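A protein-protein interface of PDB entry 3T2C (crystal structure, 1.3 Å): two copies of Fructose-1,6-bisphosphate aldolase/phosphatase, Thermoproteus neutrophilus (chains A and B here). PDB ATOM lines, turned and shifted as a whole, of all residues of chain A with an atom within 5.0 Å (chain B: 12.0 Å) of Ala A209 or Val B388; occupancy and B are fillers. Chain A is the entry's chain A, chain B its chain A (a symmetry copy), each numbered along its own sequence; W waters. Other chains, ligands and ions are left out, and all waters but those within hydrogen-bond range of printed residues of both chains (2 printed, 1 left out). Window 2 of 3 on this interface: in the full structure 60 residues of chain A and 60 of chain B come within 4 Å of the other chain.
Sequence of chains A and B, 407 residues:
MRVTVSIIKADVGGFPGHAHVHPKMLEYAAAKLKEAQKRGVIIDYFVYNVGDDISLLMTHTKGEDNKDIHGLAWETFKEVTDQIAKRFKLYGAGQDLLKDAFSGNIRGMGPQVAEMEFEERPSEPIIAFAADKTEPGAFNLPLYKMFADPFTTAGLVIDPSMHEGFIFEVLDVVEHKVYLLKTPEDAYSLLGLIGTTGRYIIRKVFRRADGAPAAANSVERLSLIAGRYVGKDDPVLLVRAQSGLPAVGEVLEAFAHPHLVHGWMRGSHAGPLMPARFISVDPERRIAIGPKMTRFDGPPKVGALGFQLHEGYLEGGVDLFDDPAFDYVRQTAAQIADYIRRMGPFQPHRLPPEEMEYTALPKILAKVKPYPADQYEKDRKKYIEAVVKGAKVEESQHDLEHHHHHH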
ATOM      1  N   GLU A 164      -4.569 -17.348  15.674  1.00  0.00           N
ATOM      2  CA  GLU A 164      -4.170 -18.693  15.263  1.00  0.00           C
ATOM      3  C   GLU A 164      -3.224 -18.738  14.086  1.00  0.00           C
ATOM      4  O   GLU A 164      -2.614 -19.780  13.845  1.00  0.00           O
ATOM      5  CB  GLU A 164      -5.346 -19.569  14.980  1.00  0.00           C
ATOM      6  CG  GLU A 164      -6.301 -19.881  16.121  1.00  0.00           C
ATOM      7  CD  GLU A 164      -7.453 -20.806  15.563  1.00  0.00           C
ATOM      8  OE1 GLU A 164      -7.152 -21.944  15.016  1.00  0.00           O
ATOM      9  OE2 GLU A 164      -8.607 -20.298  15.532  1.00  0.00           O
ATOM     10  N   GLY A 165      -3.067 -17.645  13.385  1.00  0.00           N
ATOM     11  CA  GLY A 165      -2.100 -17.570  12.330  1.00  0.00           C
ATOM     12  C   GLY A 165      -2.538 -18.028  10.965  1.00  0.00           C
ATOM     13  O   GLY A 165      -3.734 -18.126  10.636  1.00  0.00           O
ATOM     14  N   ILE A 167      -1.367 -20.124   7.001  1.00  0.00           N
ATOM     15  CA  ILE A 167      -0.695 -21.228   6.259  1.00  0.00           C
ATOM     16  C   ILE A 167      -0.193 -20.639   4.979  1.00  0.00           C
ATOM     17  O   ILE A 167      -0.944 -20.039   4.182  1.00  0.00           O
ATOM     18  CB  ILE A 167      -1.689 -22.365   5.951  1.00  0.00           C
ATOM     19  CG1 ILE A 167      -2.462 -22.811   7.197  1.00  0.00           C
ATOM     20  CG2 ILE A 167      -0.910 -23.466   5.240  1.00  0.00           C
ATOM     21  CD1 ILE A 167      -3.696 -23.686   6.906  1.00  0.00           C
ATOM     22  N   ARG A 207      -6.065 -18.827   5.860  1.00  0.00           N
ATOM     23  CA  ARG A 207      -6.259 -18.641   7.283  1.00  0.00           C
ATOM     24  C   ARG A 207      -6.216 -19.985   7.977  1.00  0.00           C
ATOM     25  O   ARG A 207      -6.874 -20.931   7.536  1.00  0.00           O
ATOM     26  CB  ARG A 207      -7.588 -17.912   7.450  1.00  0.00           C
ATOM     27  CG  ARG A 207      -7.976 -17.562   8.826  1.00  0.00           C
ATOM     28  CD  ARG A 207      -9.277 -16.708   8.819  1.00  0.00           C
ATOM     29  NE  ARG A 207      -9.520 -16.314  10.175  1.00  0.00           N
ATOM     30  CZ  ARG A 207     -10.696 -16.274  10.762  1.00  0.00           C
ATOM     31  NH1 ARG A 207     -10.749 -15.932  12.039  1.00  0.00           N
ATOM     32  NH2 ARG A 207     -11.811 -16.557  10.107  1.00  0.00           N
ATOM     33  N   ARG A 208      -5.519 -20.089   9.092  1.00  0.00           N
ATOM     34  CA  ARG A 208      -5.449 -21.336   9.790  1.00  0.00           C
ATOM     35  C   ARG A 208      -6.753 -21.719  10.498  1.00  0.00           C
ATOM     36  O   ARG A 208      -7.081 -22.923  10.616  1.00  0.00           O
ATOM     37  CB  ARG A 208      -4.297 -21.325  10.761  1.00  0.00           C
ATOM     38  CG  ARG A 208      -3.628 -22.595  10.774  1.00  0.00           C
ATOM     39  CD  ARG A 208      -3.423 -22.903  12.047  1.00  0.00           C
ATOM     40  NE  ARG A 208      -2.364 -22.143  12.600  1.00  0.00           N
ATOM     41  CZ  ARG A 208      -1.193 -22.639  12.977  1.00  0.00           C
ATOM     42  NH1 ARG A 208      -0.952 -23.939  12.885  1.00  0.00           N
ATOM     43  NH2 ARG A 208      -0.282 -21.811  13.454  1.00  0.00           N
ATOM     44  N   ALA A 209      -7.525 -20.749  10.974  1.00  0.00           N
ATOM     45  CA  ALA A 209      -8.722 -21.035  11.787  1.00  0.00           C
ATOM     46  C   ALA A 209      -9.707 -21.880  10.976  1.00  0.00           C
ATOM     47  O   ALA A 209     -10.344 -22.749  11.545  1.00  0.00           O
ATOM     48  CB  ALA A 209      -9.365 -19.703  12.182  1.00  0.00           C
ATOM     49  N   ASP A 210      -9.837 -21.625   9.685  1.00  0.00           N
ATOM     50  CA  ASP A 210     -10.898 -22.219   8.867  1.00  0.00           C
ATOM     51  C   ASP A 210     -10.426 -22.652   7.475  1.00  0.00           C
ATOM     52  O   ASP A 210     -11.267 -23.133   6.662  1.00  0.00           O
ATOM     53  CB  ASP A 210     -12.121 -21.324   8.730  1.00  0.00           C
ATOM     54  CG  ASP A 210     -11.840 -19.999   8.090  1.00  0.00           C
ATOM     55  OD1 ASP A 210     -10.664 -19.704   7.781  1.00  0.00           O
ATOM     56  OD2 ASP A 210     -12.828 -19.268   7.793  1.00  0.00           O
ATOM     57  N   GLY A 211      -9.153 -22.417   7.081  1.00  0.00           N
ATOM     58  CA  GLY A 211      -8.723 -22.670   5.742  1.00  0.00           C
ATOM     59  C   GLY A 211      -9.122 -21.658   4.701  1.00  0.00           C
ATOM     60  O   GLY A 211      -8.846 -21.942   3.520  1.00  0.00           O
ATOM     61  N   TYR B 371       6.237 -31.362  -0.969  1.00  0.00           N
ATOM     62  CA  TYR B 371       5.362 -32.130  -1.831  1.00  0.00           C
ATOM     63  C   TYR B 371       5.667 -31.856  -3.289  1.00  0.00           C
ATOM     64  O   TYR B 371       5.858 -30.748  -3.703  1.00  0.00           O
ATOM     65  CB  TYR B 371       3.930 -31.701  -1.613  1.00  0.00           C
ATOM     66  CG  TYR B 371       3.467 -31.794  -0.198  1.00  0.00           C
ATOM     67  CD1 TYR B 371       3.063 -33.000   0.319  1.00  0.00           C
ATOM     68  CD2 TYR B 371       3.398 -30.712   0.609  1.00  0.00           C
ATOM     69  CE1 TYR B 371       2.639 -33.115   1.611  1.00  0.00           C
ATOM     70  CE2 TYR B 371       2.962 -30.803   1.905  1.00  0.00           C
ATOM     71  CZ  TYR B 371       2.575 -32.003   2.412  1.00  0.00           C
ATOM     72  OH  TYR B 371       2.137 -32.047   3.706  1.00  0.00           O
ATOM     73  N   TYR B 376       0.623 -32.096  -5.579  1.00  0.00           N
ATOM     74  CA  TYR B 376       0.052 -31.189  -4.569  1.00  0.00           C
ATOM     75  C   TYR B 376      -1.173 -30.477  -5.102  1.00  0.00           C
ATOM     76  O   TYR B 376      -2.115 -30.288  -4.352  1.00  0.00           O
ATOM     77  CB  TYR B 376       1.095 -30.151  -4.242  1.00  0.00           C
ATOM     78  CG  TYR B 376       0.563 -29.076  -3.285  1.00  0.00           C
ATOM     79  CD1 TYR B 376       0.524 -29.257  -1.904  1.00  0.00           C
ATOM     80  CD2 TYR B 376       0.042 -27.883  -3.783  1.00  0.00           C
ATOM     81  CE1 TYR B 376      -0.012 -28.322  -1.052  1.00  0.00           C
ATOM     82  CE2 TYR B 376      -0.521 -26.948  -2.904  1.00  0.00           C
ATOM     83  CZ  TYR B 376      -0.547 -27.169  -1.576  1.00  0.00           C
ATOM     84  OH  TYR B 376      -1.068 -26.257  -0.694  1.00  0.00           O
ATOM     85  N   ASP B 379      -4.224 -32.437  -4.341  1.00  0.00           N
ATOM     86  CA  ASP B 379      -4.369 -32.755  -2.919  1.00  0.00           C
ATOM     87  C   ASP B 379      -4.500 -31.514  -2.029  1.00  0.00           C
ATOM     88  O   ASP B 379      -4.598 -31.634  -0.788  1.00  0.00           O
ATOM     89  CB  ASP B 379      -3.196 -33.641  -2.408  1.00  0.00           C
ATOM     90  CG  ASP B 379      -3.176 -35.041  -3.078  1.00  0.00           C
ATOM     91  OD1 ASP B 379      -4.305 -35.573  -3.380  1.00  0.00           O
ATOM     92  OD2 ASP B 379      -2.020 -35.608  -3.295  1.00  0.00           O
ATOM     93  N   ARG B 380      -4.353 -30.333  -2.622  1.00  0.00           N
ATOM     94  CA  ARG B 380      -4.264 -29.088  -1.841  1.00  0.00           C
ATOM     95  C   ARG B 380      -5.358 -28.964  -0.830  1.00  0.00           C
ATOM     96  O   ARG B 380      -5.117 -28.729   0.352  1.00  0.00           O
ATOM     97  CB  ARG B 380      -4.296 -27.875  -2.777  1.00  0.00           C
ATOM     98  CG  ARG B 380      -4.394 -26.556  -1.942  1.00  0.00           C
ATOM     99  CD  ARG B 380      -4.616 -25.318  -2.829  1.00  0.00           C
ATOM    100  NE  ARG B 380      -3.457 -24.901  -3.610  1.00  0.00           N
ATOM    101  CZ  ARG B 380      -3.279 -24.974  -4.910  1.00  0.00           C
ATOM    102  NH1 ARG B 380      -4.200 -25.627  -5.679  1.00  0.00           N
ATOM    103  NH2 ARG B 380      -2.166 -24.559  -5.452  1.00  0.00           N
ATOM    104  N   LYS B 381      -6.606 -29.176  -1.244  1.00  0.00           N
ATOM    105  CA  LYS B 381      -7.692 -29.099  -0.272  1.00  0.00           C
ATOM    106  C   LYS B 381      -7.548 -30.033   0.893  1.00  0.00           C
ATOM    107  O   LYS B 381      -7.751 -29.646   1.989  1.00  0.00           O
ATOM    108  CB  LYS B 381      -9.076 -29.298  -0.896  1.00  0.00           C
ATOM    109  CG  LYS B 381      -9.332 -28.457  -2.084  1.00  0.00           C
ATOM    110  CD  LYS B 381     -10.716 -28.678  -2.731  1.00  0.00           C
ATOM    111  CE  LYS B 381     -10.822 -30.009  -3.582  1.00  0.00           C
ATOM    112  NZ  LYS B 381      -9.944 -30.032  -4.805  1.00  0.00           N
ATOM    113  N   LYS B 382      -7.226 -31.288   0.636  1.00  0.00           N
ATOM    114  CA  LYS B 382      -6.998 -32.173   1.813  1.00  0.00           C
ATOM    115  C   LYS B 382      -5.847 -31.818   2.664  1.00  0.00           C
ATOM    116  O   LYS B 382      -5.942 -31.952   3.907  1.00  0.00           O
ATOM    117  CB  LYS B 382      -6.778 -33.672   1.483  1.00  0.00           C
ATOM    118  CG  LYS B 382      -6.521 -33.913   0.080  1.00  0.00           C
ATOM    119  CD  LYS B 382      -7.873 -34.103  -0.607  1.00  0.00           C
ATOM    120  CE  LYS B 382      -7.791 -33.739  -2.090  1.00  0.00           C
ATOM    121  NZ  LYS B 382      -7.816 -32.288  -2.245  1.00  0.00           N
ATOM    122  N   TYR B 383      -4.756 -31.305   2.081  1.00  0.00           N
ATOM    123  CA  TYR B 383      -3.647 -30.868   2.950  1.00  0.00           C
ATOM    124  C   TYR B 383      -3.999 -29.697   3.796  1.00  0.00           C
ATOM    125  O   TYR B 383      -3.628 -29.651   5.010  1.00  0.00           O
ATOM    126  CB  TYR B 383      -2.456 -30.521   2.170  1.00  0.00           C
ATOM    127  CG  TYR B 383      -1.793 -31.679   1.538  1.00  0.00           C
ATOM    128  CD1 TYR B 383      -1.716 -32.910   2.155  1.00  0.00           C
ATOM    129  CD2 TYR B 383      -1.336 -31.587   0.263  1.00  0.00           C
ATOM    130  CE1 TYR B 383      -1.092 -34.004   1.498  1.00  0.00           C
ATOM    131  CE2 TYR B 383      -0.740 -32.615  -0.380  1.00  0.00           C
ATOM    132  CZ  TYR B 383      -0.615 -33.841   0.207  1.00  0.00           C
ATOM    133  OH  TYR B 383       0.025 -34.863  -0.494  1.00  0.00           O
ATOM    134  N   ILE B 384      -4.679 -28.706   3.205  1.00  0.00           N
ATOM    135  CA  ILE B 384      -5.072 -27.532   3.988  1.00  0.00           C
ATOM    136  C   ILE B 384      -6.036 -27.953   5.105  1.00  0.00           C
ATOM    137  O   ILE B 384      -5.860 -27.544   6.243  1.00  0.00           O
ATOM    138  CB  ILE B 384      -5.605 -26.330   3.107  1.00  0.00           C
ATOM    139  CG1 ILE B 384      -4.588 -25.875   2.044  1.00  0.00           C
ATOM    140  CG2 ILE B 384      -5.975 -25.151   4.010  1.00  0.00           C
ATOM    141  CD1 ILE B 384      -3.269 -25.255   2.603  1.00  0.00           C
ATOM    142  N   GLU B 385      -7.038 -28.799   4.787  1.00  0.00           N
ATOM    143  CA  GLU B 385      -7.954 -29.257   5.826  1.00  0.00           C
ATOM    144  C   GLU B 385      -7.223 -30.013   6.926  1.00  0.00           C
ATOM    145  O   GLU B 385      -7.563 -29.842   8.072  1.00  0.00           O
ATOM    146  CB  GLU B 385      -9.065 -30.158   5.269  1.00  0.00           C
ATOM    147  CG  GLU B 385     -10.007 -29.423   4.370  1.00  0.00           C
ATOM    148  CD  GLU B 385     -11.051 -30.331   3.632  1.00  0.00           C
ATOM    149  OE1 GLU B 385     -11.137 -31.560   3.902  1.00  0.00           O
ATOM    150  OE2 GLU B 385     -11.786 -29.773   2.753  1.00  0.00           O
ATOM    151  N   ALA B 386      -6.184 -30.776   6.597  1.00  0.00           N
ATOM    152  CA  ALA B 386      -5.367 -31.445   7.624  1.00  0.00           C
ATOM    153  C   ALA B 386      -4.658 -30.482   8.549  1.00  0.00           C
ATOM    154  O   ALA B 386      -4.689 -30.654   9.771  1.00  0.00           O
ATOM    155  CB  ALA B 386      -4.368 -32.415   6.949  1.00  0.00           C
ATOM    156  N   VAL B 387      -4.086 -29.414   7.977  1.00  0.00           N
ATOM    157  CA  VAL B 387      -3.476 -28.411   8.817  1.00  0.00           C
ATOM    158  C   VAL B 387      -4.531 -27.733   9.710  1.00  0.00           C
ATOM    159  O   VAL B 387      -4.292 -27.443  10.910  1.00  0.00           O
ATOM    160  CB  VAL B 387      -2.733 -27.361   7.964  1.00  0.00           C
ATOM    161  CG1 VAL B 387      -2.184 -26.236   8.873  1.00  0.00           C
ATOM    162  CG2 VAL B 387      -1.631 -28.047   7.145  1.00  0.00           C
ATOM    163  N   VAL B 388      -5.673 -27.354   9.116  1.00  0.00           N
ATOM    164  CA  VAL B 388      -6.705 -26.722   9.871  1.00  0.00           C
ATOM    165  C   VAL B 388      -7.168 -27.608  11.067  1.00  0.00           C
ATOM    166  O   VAL B 388      -7.338 -27.112  12.179  1.00  0.00           O
ATOM    167  CB  VAL B 388      -7.856 -26.298   8.942  1.00  0.00           C
ATOM    168  CG1 VAL B 388      -9.012 -25.759   9.729  1.00  0.00           C
ATOM    169  CG2 VAL B 388      -7.357 -25.207   7.876  1.00  0.00           C
ATOM    170  N   LYS B 389      -7.380 -28.890  10.859  1.00  0.00           N
ATOM    171  CA  LYS B 389      -7.886 -29.743  11.944  1.00  0.00           C
ATOM    172  C   LYS B 389      -6.814 -30.264  12.894  1.00  0.00           C
ATOM    173  O   LYS B 389      -5.628 -30.097  12.665  1.00  0.00           O
ATOM    174  CB  LYS B 389      -8.683 -30.879  11.351  1.00  0.00           C
ATOM    175  CG  LYS B 389      -9.933 -30.396  10.641  1.00  0.00           C
ATOM    176  CD  LYS B 389     -10.213 -31.319   9.464  1.00  0.00           C
ATOM    177  CE  LYS B 389     -11.701 -31.413   9.144  1.00  0.00           C
ATOM    178  NZ  LYS B 389     -11.853 -31.855   7.740  1.00  0.00           N
HETATM  179  O   HOH W   1      -1.991 -26.605  13.142  1.00  0.00           O
HETATM  180  O   HOH W   2      -6.527 -24.617  12.747  1.00  0.00           O
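The backbone carbonyl oxygen of Glu A164 lies within hydrogen-bond range of the guanidinium group of Arg A208. The backbone NH (N) of Arg A208 lies within hydrogen-bond range of the backbone carbonyl oxygen (O) of Gly A165, 3.1 Å away.
Among the printed residues, merely in contact across the chains: Gly A211 with Val B388, Arg A208 with Val B388, Ile A167 with Val B387, Ala A209 with Val B388 and Ile A167 with Ile B384.
No residue of chain B comes within 4 Å of Glu A164. Of the printed residues of chain B, Arg A208 touches Val B388. Ala A209 touches one residue of chain B. Of the printed residues of chain B, Gly A211 touches Val B388 (3.4 Å). Tyr B383 touches none of the printed residues of chain A. Printed residues of chain A within 4 Å of Ile B384: Ile A167. Glu B385 touches none of the printed residues of chain A. Printed residues of chain A within 4 Å of Val B387: Ile A167. Of the printed residues of chain A, Val B388 touches Arg A208 (3.5 Å), Ala A209 (3.8 Å) and Gly A211 (3.4 Å). The nearest residue of chain B that does not touch Ala A209 is Lys B389 (6.9 Å).
Of the 8 printed residues of chain A, 4 touch a printed residue of chain B. Hydrophobic or aromatic side chains of chain A that line the printed part of chain B: Ile A167. Along chain A the printed residues that touch a printed residue of chain B span positions 167 to 211. Hydrophobic or aromatic side chains of chain B within 4 Å of the printed part of chain A: Ile B384, Val B387 and Val B388. Among the printed residues, no Asp or Glu carboxylate lies within 4 Å of a Lys or Arg side-chain nitrogen of the other chain.
No position is printed for both chains. Of the 5 pairs that touch across the chains among the printed residues, none has its exchanged pair printed and touching as well.
Water W2 lies within hydrogen-bond range of O of Val B388 and O of Arg A208. Water W1 bridges NH1 of Arg A208 (2.9 Å) and O of Val B387 (3.3 Å).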
